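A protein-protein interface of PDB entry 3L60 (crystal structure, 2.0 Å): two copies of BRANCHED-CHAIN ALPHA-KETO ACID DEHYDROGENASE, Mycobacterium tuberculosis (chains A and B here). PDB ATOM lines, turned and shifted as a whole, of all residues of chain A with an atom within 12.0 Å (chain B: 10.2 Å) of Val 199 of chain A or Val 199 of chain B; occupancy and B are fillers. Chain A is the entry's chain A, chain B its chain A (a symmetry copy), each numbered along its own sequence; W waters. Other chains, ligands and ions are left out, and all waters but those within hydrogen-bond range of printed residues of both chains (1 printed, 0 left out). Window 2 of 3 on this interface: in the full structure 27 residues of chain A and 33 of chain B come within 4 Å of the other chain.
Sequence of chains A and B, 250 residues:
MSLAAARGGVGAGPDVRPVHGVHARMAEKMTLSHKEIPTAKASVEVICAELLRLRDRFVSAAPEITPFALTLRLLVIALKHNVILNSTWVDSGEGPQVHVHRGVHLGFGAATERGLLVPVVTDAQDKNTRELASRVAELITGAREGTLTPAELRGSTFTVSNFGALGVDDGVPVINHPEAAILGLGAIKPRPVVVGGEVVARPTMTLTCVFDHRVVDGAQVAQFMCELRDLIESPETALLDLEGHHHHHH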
ATOM      1  N   GLU A  45      35.957 -16.447  28.690  1.00  0.00           N
ATOM      2  CA  GLU A  45      35.310 -16.407  27.408  1.00  0.00           C
ATOM      3  C   GLU A  45      34.296 -15.251  27.448  1.00  0.00           C
ATOM      4  O   GLU A  45      33.573 -15.105  28.429  1.00  0.00           O
ATOM      5  CB  GLU A  45      34.584 -17.733  27.146  1.00  0.00           C
ATOM      6  CG  GLU A  45      33.928 -17.794  25.765  1.00  0.00           C
ATOM      7  CD  GLU A  45      33.390 -19.198  25.411  1.00  0.00           C
ATOM      8  OE1 GLU A  45      32.531 -19.714  26.194  1.00  0.00           O
ATOM      9  OE2 GLU A  45      33.834 -19.774  24.358  1.00  0.00           O
ATOM     10  N   ILE A  47      31.272 -13.159  25.131  1.00  0.00           N
ATOM     11  CA  ILE A  47      30.390 -13.051  23.964  1.00  0.00           C
ATOM     12  C   ILE A  47      30.398 -11.605  23.382  1.00  0.00           C
ATOM     13  O   ILE A  47      30.166 -10.638  24.104  1.00  0.00           O
ATOM     14  CB  ILE A  47      28.971 -13.470  24.345  1.00  0.00           C
ATOM     15  CG1 ILE A  47      28.967 -14.933  24.856  1.00  0.00           C
ATOM     16  CG2 ILE A  47      28.055 -13.284  23.145  1.00  0.00           C
ATOM     17  CD1 ILE A  47      27.676 -15.382  25.650  1.00  0.00           C
ATOM     18  N   LYS A 189      35.460 -14.636  16.618  1.00  0.00           N
ATOM     19  CA  LYS A 189      34.761 -15.332  15.539  1.00  0.00           C
ATOM     20  C   LYS A 189      33.553 -16.048  16.111  1.00  0.00           C
ATOM     21  O   LYS A 189      33.445 -16.201  17.340  1.00  0.00           O
ATOM     22  CB  LYS A 189      35.690 -16.311  14.759  1.00  0.00           C
ATOM     23  CG  LYS A 189      35.941 -17.638  15.424  1.00  0.00           C
ATOM     24  CD  LYS A 189      37.196 -18.354  14.856  1.00  0.00           C
ATOM     25  CE  LYS A 189      37.179 -19.832  15.188  1.00  0.00           C
ATOM     26  NZ  LYS A 189      38.538 -20.453  15.156  1.00  0.00           N
ATOM     27  N   PRO A 190      32.652 -16.520  15.222  1.00  0.00           N
ATOM     28  CA  PRO A 190      31.541 -17.347  15.683  1.00  0.00           C
ATOM     29  C   PRO A 190      31.994 -18.659  16.322  1.00  0.00           C
ATOM     30  O   PRO A 190      32.724 -19.442  15.705  1.00  0.00           O
ATOM     31  CB  PRO A 190      30.765 -17.653  14.394  1.00  0.00           C
ATOM     32  CG  PRO A 190      31.267 -16.717  13.367  1.00  0.00           C
ATOM     33  CD  PRO A 190      32.676 -16.414  13.750  1.00  0.00           C
ATOM     34  N   ARG A 191      31.534 -18.893  17.541  1.00  0.00           N
ATOM     35  CA  ARG A 191      31.729 -20.148  18.209  1.00  0.00           C
ATOM     36  C   ARG A 191      30.423 -20.515  18.916  1.00  0.00           C
ATOM     37  O   ARG A 191      29.597 -19.642  19.215  1.00  0.00           O
ATOM     38  CB  ARG A 191      32.862 -20.034  19.244  1.00  0.00           C
ATOM     39  CG  ARG A 191      34.167 -19.526  18.671  1.00  0.00           C
ATOM     40  CD  ARG A 191      35.314 -19.753  19.617  1.00  0.00           C
ATOM     41  NE  ARG A 191      36.582 -19.349  19.010  1.00  0.00           N
ATOM     42  CZ  ARG A 191      37.005 -18.093  18.881  1.00  0.00           C
ATOM     43  NH1 ARG A 191      36.272 -17.068  19.268  1.00  0.00           N
ATOM     44  NH2 ARG A 191      38.163 -17.845  18.311  1.00  0.00           N
ATOM     45  N   PRO A 192      30.251 -21.800  19.221  1.00  0.00           N
ATOM     46  CA  PRO A 192      29.069 -22.239  19.971  1.00  0.00           C
ATOM     47  C   PRO A 192      29.111 -21.834  21.427  1.00  0.00           C
ATOM     48  O   PRO A 192      30.151 -21.985  22.089  1.00  0.00           O
ATOM     49  CB  PRO A 192      29.154 -23.775  19.888  1.00  0.00           C
ATOM     50  CG  PRO A 192      30.071 -24.049  18.739  1.00  0.00           C
ATOM     51  CD  PRO A 192      31.083 -22.953  18.839  1.00  0.00           C
ATOM     52  N   VAL A 193      27.997 -21.319  21.928  1.00  0.00           N
ATOM     53  CA  VAL A 193      27.852 -21.031  23.343  1.00  0.00           C
ATOM     54  C   VAL A 193      26.430 -21.431  23.766  1.00  0.00           C
ATOM     55  O   VAL A 193      25.562 -21.657  22.898  1.00  0.00           O
ATOM     56  CB  VAL A 193      28.129 -19.560  23.706  1.00  0.00           C
ATOM     57  CG1 VAL A 193      29.596 -19.140  23.375  1.00  0.00           C
ATOM     58  CG2 VAL A 193      27.069 -18.595  23.065  1.00  0.00           C
ATOM     59  N   VAL A 194      26.203 -21.552  25.070  1.00  0.00           N
ATOM     60  CA  VAL A 194      24.855 -21.784  25.594  1.00  0.00           C
ATOM     61  C   VAL A 194      24.252 -20.461  26.050  1.00  0.00           C
ATOM     62  O   VAL A 194      24.842 -19.751  26.844  1.00  0.00           O
ATOM     63  CB  VAL A 194      24.864 -22.777  26.747  1.00  0.00           C
ATOM     64  CG1 VAL A 194      23.436 -22.996  27.334  1.00  0.00           C
ATOM     65  CG2 VAL A 194      25.538 -24.092  26.301  1.00  0.00           C
ATOM     66  N   VAL A 195      23.069 -20.131  25.534  1.00  0.00           N
ATOM     67  CA  VAL A 195      22.334 -18.932  25.962  1.00  0.00           C
ATOM     68  C   VAL A 195      20.905 -19.397  26.275  1.00  0.00           C
ATOM     69  O   VAL A 195      20.267 -20.055  25.446  1.00  0.00           O
ATOM     70  CB  VAL A 195      22.332 -17.849  24.872  1.00  0.00           C
ATOM     71  CG1 VAL A 195      21.559 -16.563  25.352  1.00  0.00           C
ATOM     72  CG2 VAL A 195      23.764 -17.502  24.453  1.00  0.00           C
ATOM     73  N   GLY A 196      20.467 -19.150  27.502  1.00  0.00           N
ATOM     74  CA  GLY A 196      19.148 -19.589  27.979  1.00  0.00           C
ATOM     75  C   GLY A 196      18.904 -21.054  27.715  1.00  0.00           C
ATOM     76  O   GLY A 196      17.841 -21.442  27.215  1.00  0.00           O
ATOM     77  N   GLY A 197      19.938 -21.851  27.964  1.00  0.00           N
ATOM     78  CA  GLY A 197      19.863 -23.290  27.852  1.00  0.00           C
ATOM     79  C   GLY A 197      19.899 -23.861  26.455  1.00  0.00           C
ATOM     80  O   GLY A 197      19.823 -25.071  26.305  1.00  0.00           O
ATOM     81  N   GLU A 198      20.012 -23.012  25.437  1.00  0.00           N
ATOM     82  CA  GLU A 198      20.087 -23.447  24.040  1.00  0.00           C
ATOM     83  C   GLU A 198      21.517 -23.257  23.502  1.00  0.00           C
ATOM     84  O   GLU A 198      22.128 -22.217  23.736  1.00  0.00           O
ATOM     85  CB  GLU A 198      19.164 -22.594  23.150  1.00  0.00           C
ATOM     86  CG  GLU A 198      17.707 -22.470  23.622  1.00  0.00           C
ATOM     87  CD  GLU A 198      16.917 -23.772  23.484  1.00  0.00           C
ATOM     88  OE1 GLU A 198      17.291 -24.620  22.640  1.00  0.00           O
ATOM     89  OE2 GLU A 198      15.910 -23.941  24.218  1.00  0.00           O
ATOM     90  N   VAL A 199      22.008 -24.218  22.726  1.00  0.00           N
ATOM     91  CA  VAL A 199      23.284 -24.028  22.021  1.00  0.00           C
ATOM     92  C   VAL A 199      23.075 -23.146  20.799  1.00  0.00           C
ATOM     93  O   VAL A 199      22.291 -23.489  19.904  1.00  0.00           O
ATOM     94  CB  VAL A 199      23.914 -25.376  21.618  1.00  0.00           C
ATOM     95  CG1 VAL A 199      25.252 -25.163  20.915  1.00  0.00           C
ATOM     96  CG2 VAL A 199      24.082 -26.248  22.850  1.00  0.00           C
ATOM     97  N   VAL A 200      23.771 -22.011  20.767  1.00  0.00           N
ATOM     98  CA  VAL A 200      23.650 -21.015  19.702  1.00  0.00           C
ATOM     99  C   VAL A 200      25.016 -20.593  19.195  1.00  0.00           C
ATOM    100  O   VAL A 200      26.009 -20.804  19.869  1.00  0.00           O
ATOM    101  CB  VAL A 200      22.900 -19.738  20.169  1.00  0.00           C
ATOM    102  CG1 VAL A 200      21.401 -20.080  20.420  1.00  0.00           C
ATOM    103  CG2 VAL A 200      23.543 -19.082  21.411  1.00  0.00           C
ATOM    104  N   ALA A 201      25.056 -20.037  17.991  1.00  0.00           N
ATOM    105  CA  ALA A 201      26.259 -19.407  17.486  1.00  0.00           C
ATOM    106  C   ALA A 201      26.326 -17.958  17.957  1.00  0.00           C
ATOM    107  O   ALA A 201      25.316 -17.220  17.924  1.00  0.00           O
ATOM    108  CB  ALA A 201      26.329 -19.472  15.969  1.00  0.00           C
ATOM    109  N   ARG A 202      27.521 -17.552  18.407  1.00  0.00           N
ATOM    110  CA  ARG A 202      27.801 -16.160  18.736  1.00  0.00           C
ATOM    111  C   ARG A 202      29.245 -15.810  18.372  1.00  0.00           C
ATOM    112  O   ARG A 202      30.142 -16.660  18.497  1.00  0.00           O
ATOM    113  CB  ARG A 202      27.623 -15.870  20.231  1.00  0.00           C
ATOM    114  CG  ARG A 202      26.230 -15.962  20.793  1.00  0.00           C
ATOM    115  CD  ARG A 202      25.301 -14.846  20.217  1.00  0.00           C
ATOM    116  NE  ARG A 202      24.009 -14.917  20.894  1.00  0.00           N
ATOM    117  CZ  ARG A 202      22.955 -15.621  20.468  1.00  0.00           C
ATOM    118  NH1 ARG A 202      22.981 -16.292  19.315  1.00  0.00           N
ATOM    119  NH2 ARG A 202      21.852 -15.631  21.197  1.00  0.00           N
ATOM    120  N   PRO A 203      29.484 -14.545  17.976  1.00  0.00           N
ATOM    121  CA  PRO A 203      30.883 -14.102  17.946  1.00  0.00           C
ATOM    122  C   PRO A 203      31.425 -14.069  19.366  1.00  0.00           C
ATOM    123  O   PRO A 203      30.773 -13.544  20.270  1.00  0.00           O
ATOM    124  CB  PRO A 203      30.811 -12.699  17.355  1.00  0.00           C
ATOM    125  CG  PRO A 203      29.368 -12.233  17.638  1.00  0.00           C
ATOM    126  CD  PRO A 203      28.529 -13.472  17.610  1.00  0.00           C
ATOM    127  N   THR A 204      32.597 -14.665  19.576  1.00  0.00           N
ATOM    128  CA  THR A 204      33.175 -14.733  20.920  1.00  0.00           C
ATOM    129  C   THR A 204      34.655 -14.476  20.849  1.00  0.00           C
ATOM    130  O   THR A 204      35.258 -14.512  19.751  1.00  0.00           O
ATOM    131  CB  THR A 204      32.952 -16.118  21.630  1.00  0.00           C
ATOM    132  OG1 THR A 204      33.760 -17.135  21.023  1.00  0.00           O
ATOM    133  CG2 THR A 204      31.477 -16.559  21.583  1.00  0.00           C
ATOM    134  N   ARG B 191      33.881 -32.044  18.740  1.00  0.00           N
ATOM    135  CA  ARG B 191      33.503 -30.905  19.528  1.00  0.00           C
ATOM    136  C   ARG B 191      32.600 -30.017  18.671  1.00  0.00           C
ATOM    137  O   ARG B 191      32.641 -30.076  17.435  1.00  0.00           O
ATOM    138  CB  ARG B 191      34.750 -30.113  19.958  1.00  0.00           C
ATOM    139  CG  ARG B 191      35.785 -30.944  20.683  1.00  0.00           C
ATOM    140  CD  ARG B 191      36.805 -30.080  21.373  1.00  0.00           C
ATOM    141  NE  ARG B 191      37.740 -30.893  22.152  1.00  0.00           N
ATOM    142  CZ  ARG B 191      38.751 -31.595  21.646  1.00  0.00           C
ATOM    143  NH1 ARG B 191      38.982 -31.650  20.349  1.00  0.00           N
ATOM    144  NH2 ARG B 191      39.527 -32.298  22.442  1.00  0.00           N
ATOM    145  N   PRO B 192      31.812 -29.164  19.323  1.00  0.00           N
ATOM    146  CA  PRO B 192      30.969 -28.213  18.588  1.00  0.00           C
ATOM    147  C   PRO B 192      31.760 -27.094  17.951  1.00  0.00           C
ATOM    148  O   PRO B 192      32.649 -26.511  18.594  1.00  0.00           O
ATOM    149  CB  PRO B 192      30.075 -27.615  19.691  1.00  0.00           C
ATOM    150  CG  PRO B 192      30.158 -28.587  20.824  1.00  0.00           C
ATOM    151  CD  PRO B 192      31.577 -29.055  20.772  1.00  0.00           C
ATOM    152  N   VAL B 193      31.452 -26.794  16.698  1.00  0.00           N
ATOM    153  CA  VAL B 193      32.024 -25.646  16.019  1.00  0.00           C
ATOM    154  C   VAL B 193      30.917 -24.988  15.181  1.00  0.00           C
ATOM    155  O   VAL B 193      29.851 -25.601  14.964  1.00  0.00           O
ATOM    156  CB  VAL B 193      33.237 -25.992  15.134  1.00  0.00           C
ATOM    157  CG1 VAL B 193      34.421 -26.580  15.965  1.00  0.00           C
ATOM    158  CG2 VAL B 193      32.831 -26.915  13.930  1.00  0.00           C
ATOM    159  N   VAL B 194      31.145 -23.752  14.748  1.00  0.00           N
ATOM    160  CA  VAL B 194      30.229 -23.084  13.822  1.00  0.00           C
ATOM    161  C   VAL B 194      30.756 -23.218  12.398  1.00  0.00           C
ATOM    162  O   VAL B 194      31.887 -22.865  12.120  1.00  0.00           O
ATOM    163  CB  VAL B 194      30.047 -21.614  14.174  1.00  0.00           C
ATOM    164  CG1 VAL B 194      29.103 -20.890  13.166  1.00  0.00           C
ATOM    165  CG2 VAL B 194      29.579 -21.480  15.638  1.00  0.00           C
ATOM    166  N   VAL B 195      29.924 -23.739  11.497  1.00  0.00           N
ATOM    167  CA  VAL B 195      30.273 -23.834  10.072  1.00  0.00           C
ATOM    168  C   VAL B 195      29.082 -23.245   9.303  1.00  0.00           C
ATOM    169  O   VAL B 195      27.935 -23.649   9.522  1.00  0.00           O
ATOM    170  CB  VAL B 195      30.536 -25.288   9.648  1.00  0.00           C
ATOM    171  CG1 VAL B 195      30.927 -25.371   8.124  1.00  0.00           C
ATOM    172  CG2 VAL B 195      31.620 -25.919  10.527  1.00  0.00           C
ATOM    173  N   GLY B 196      29.354 -22.226   8.500  1.00  0.00           N
ATOM    174  CA  GLY B 196      28.315 -21.510   7.743  1.00  0.00           C
ATOM    175  C   GLY B 196      27.166 -21.081   8.620  1.00  0.00           C
ATOM    176  O   GLY B 196      25.994 -21.279   8.276  1.00  0.00           O
ATOM    177  N   GLY B 197      27.514 -20.581   9.801  1.00  0.00           N
ATOM    178  CA  GLY B 197      26.554 -20.039  10.736  1.00  0.00           C
ATOM    179  C   GLY B 197      25.740 -21.038  11.522  1.00  0.00           C
ATOM    180  O   GLY B 197      24.904 -20.631  12.315  1.00  0.00           O
ATOM    181  N   GLU B 198      25.970 -22.331  11.314  1.00  0.00           N
ATOM    182  CA  GLU B 198      25.265 -23.393  12.036  1.00  0.00           C
ATOM    183  C   GLU B 198      26.211 -24.061  13.051  1.00  0.00           C
ATOM    184  O   GLU B 198      27.357 -24.357  12.720  1.00  0.00           O
ATOM    185  CB  GLU B 198      24.803 -24.499  11.070  1.00  0.00           C
ATOM    186  CG  GLU B 198      24.003 -24.027   9.846  1.00  0.00           C
ATOM    187  CD  GLU B 198      22.605 -23.518  10.200  1.00  0.00           C
ATOM    188  OE1 GLU B 198      22.063 -23.924  11.255  1.00  0.00           O
ATOM    189  OE2 GLU B 198      22.044 -22.714   9.412  1.00  0.00           O
ATOM    190  N   VAL B 199      25.707 -24.366  14.243  1.00  0.00           N
ATOM    191  CA  VAL B 199      26.484 -25.172  15.197  1.00  0.00           C
ATOM    192  C   VAL B 199      26.431 -26.640  14.799  1.00  0.00           C
ATOM    193  O   VAL B 199      25.346 -27.231  14.725  1.00  0.00           O
ATOM    194  CB  VAL B 199      25.980 -24.982  16.641  1.00  0.00           C
ATOM    195  CG1 VAL B 199      26.815 -25.801  17.621  1.00  0.00           C
ATOM    196  CG2 VAL B 199      26.014 -23.507  17.002  1.00  0.00           C
ATOM    197  N   VAL B 200      27.600 -27.221  14.536  1.00  0.00           N
ATOM    198  CA  VAL B 200      27.734 -28.604  14.080  1.00  0.00           C
ATOM    199  C   VAL B 200      28.785 -29.343  14.888  1.00  0.00           C
ATOM    200  O   VAL B 200      29.608 -28.718  15.534  1.00  0.00           O
ATOM    201  CB  VAL B 200      28.133 -28.697  12.582  1.00  0.00           C
ATOM    202  CG1 VAL B 200      26.944 -28.213  11.699  1.00  0.00           C
ATOM    203  CG2 VAL B 200      29.429 -27.924  12.254  1.00  0.00           C
ATOM    204  N   ALA B 201      28.720 -30.668  14.874  1.00  0.00           N
ATOM    205  CA  ALA B 201      29.780 -31.485  15.429  1.00  0.00           C
ATOM    206  C   ALA B 201      30.868 -31.710  14.384  1.00  0.00           C
ATOM    207  O   ALA B 201      30.577 -31.993  13.200  1.00  0.00           O
ATOM    208  CB  ALA B 201      29.252 -32.817  15.935  1.00  0.00           C
ATOM    209  N   ARG B 202      32.126 -31.573  14.822  1.00  0.00           N
ATOM    210  CA  ARG B 202      33.281 -31.915  14.001  1.00  0.00           C
ATOM    211  C   ARG B 202      34.395 -32.499  14.872  1.00  0.00           C
ATOM    212  O   ARG B 202      34.570 -32.077  16.027  1.00  0.00           O
ATOM    213  CB  ARG B 202      33.860 -30.694  13.277  1.00  0.00           C
ATOM    214  CG  ARG B 202      33.009 -30.050  12.216  1.00  0.00           C
ATOM    215  CD  ARG B 202      32.811 -30.992  10.985  1.00  0.00           C
ATOM    216  NE  ARG B 202      32.085 -30.261   9.950  1.00  0.00           N
ATOM    217  CZ  ARG B 202      30.756 -30.255   9.801  1.00  0.00           C
ATOM    218  NH1 ARG B 202      29.961 -30.991  10.580  1.00  0.00           N
ATOM    219  NH2 ARG B 202      30.221 -29.520   8.842  1.00  0.00           N
HETATM  220  O   HOH W   1      33.398 -22.154  15.778  1.00  0.00           O
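The backbone NH of Arg 191 of chain A lies within hydrogen-bond range of the backbone carbonyl oxygen of Arg 202 of chain A. The backbone carbonyl oxygen of Val 193 of chain B lies within hydrogen-bond range of the backbone NH of Val 200 of chain B (2.8 Å). The guanidinium group (NH1) of Arg 191 of chain A is in hydrogen-bond range of the backbone carbonyl oxygen (O) of Thr 204 of chain A (2.8 Å). The backbone NH of Val 200 of chain A lies within hydrogen-bond range of the backbone carbonyl oxygen of Val 193 of chain A, at 2.8 Å.
Val 194 of chain B touches Pro 190 of chain A. CG2 of Val 194 of chain B touches C of Arg 191 of chain A, 3.5 Å away. CG of Pro 192 of chain A touches O of Pro 192 of chain B (3.6 Å). Pro 192 of chain A touches Val 193 of chain B. Pro 192 of chain A touches Val 194 of chain B (N to CG2, 3.7 Å). CG1 of Val 199 of chain B touches CB of Pro 192 of chain A, at 3.8 Å. Val 199 of chain A touches Val 199 of chain B (CG1 to CG1, 3.7 Å). Val 199 of chain B touches Val 200 of chain A (CG2 to C, 3.8 Å). Ala 201 of chain A touches Val 194 of chain B (CB to CG2, 3.8 Å). Ala 201 of chain A touches Val 199 of chain B.
Printed residues of chain B within 4 Å of Pro 190 of chain A: Val 194. Of the printed residues of chain B, Arg 191 of chain A touches Val 194. Pro 192 of chain A touches four residues of chain B. Printed residues of chain B within 4 Å of Ala 201 of chain A: Val 194 (3.8 Å) and Val 199 (3.7 Å). Arg 202 of chain A touches none of the printed residues of chain B. Of chain A, only Pro 192 (3.6 Å) comes within 4 Å of Pro 192 of chain B. Val 194 of chain B touches just these residues of chain A: Pro 190 (3.7 Å), Arg 191 (3.5 Å), Pro 192 (3.7 Å) and Ala 201 (3.8 Å). No residue of chain A comes within 4 Å of Gly 196 of chain B. No residue of chain A comes within 4 Å of Gly 197 of chain B. Glu 198 of chain B touches none of the printed residues of chain A. Val 199 of chain B touches just these residues of chain A: Pro 192 (3.8 Å), Val 199 (3.7 Å), Val 200 (3.8 Å) and Ala 201 (3.7 Å). No residue of chain A comes within 4 Å of Val 200 of chain B. The nearest residue of chain B that does not touch Val 199 of chain A is Pro 192 of chain B (5.5 Å).
Of the 18 printed residues of chain A, 6 touch a printed residue of chain B. Printed residues of chain A that touch a printed residue of chain B: Pro 190, Arg 191, Pro 192, Val 199, Val 200 and Ala 201. Hydrophobic or aromatic side chains of chain B within 4 Å of the printed part of chain A: Pro 192, Val 194 and Val 199. Among the printed residues, 10 pairs touch across the chains. Among the printed residues, no Asp or Glu carboxylate lies within 4 Å of a Lys or Arg side-chain nitrogen of the other chain.
Arg 191 of chain A touches Val 194 of chain B, but with the chains exchanged Val 194 of chain A does not touch Arg 191 of chain B (12.0 Å). Pro 192 of chain A touches Val 199 of chain B, but with the chains exchanged Val 199 of chain A does not touch Pro 192 of chain B (5.5 Å). Val 199 of chain A touches its own counterpart, Val 199 of chain B. Ala 201 of chain A touches Val 199 of chain B, but with the chains exchanged Val 199 of chain A does not touch Ala 201 of chain B (8.9 Å). 12 positions are printed for both chains. Of the 10 pairs that touch across the chains among the printed residues, 2 have their exchanged pair printed and touching as well.
Water W1 lies within hydrogen-bond range of O of Pro 190 of chain A (2.8 Å) and N of Val 194 of chain B (2.9 Å).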
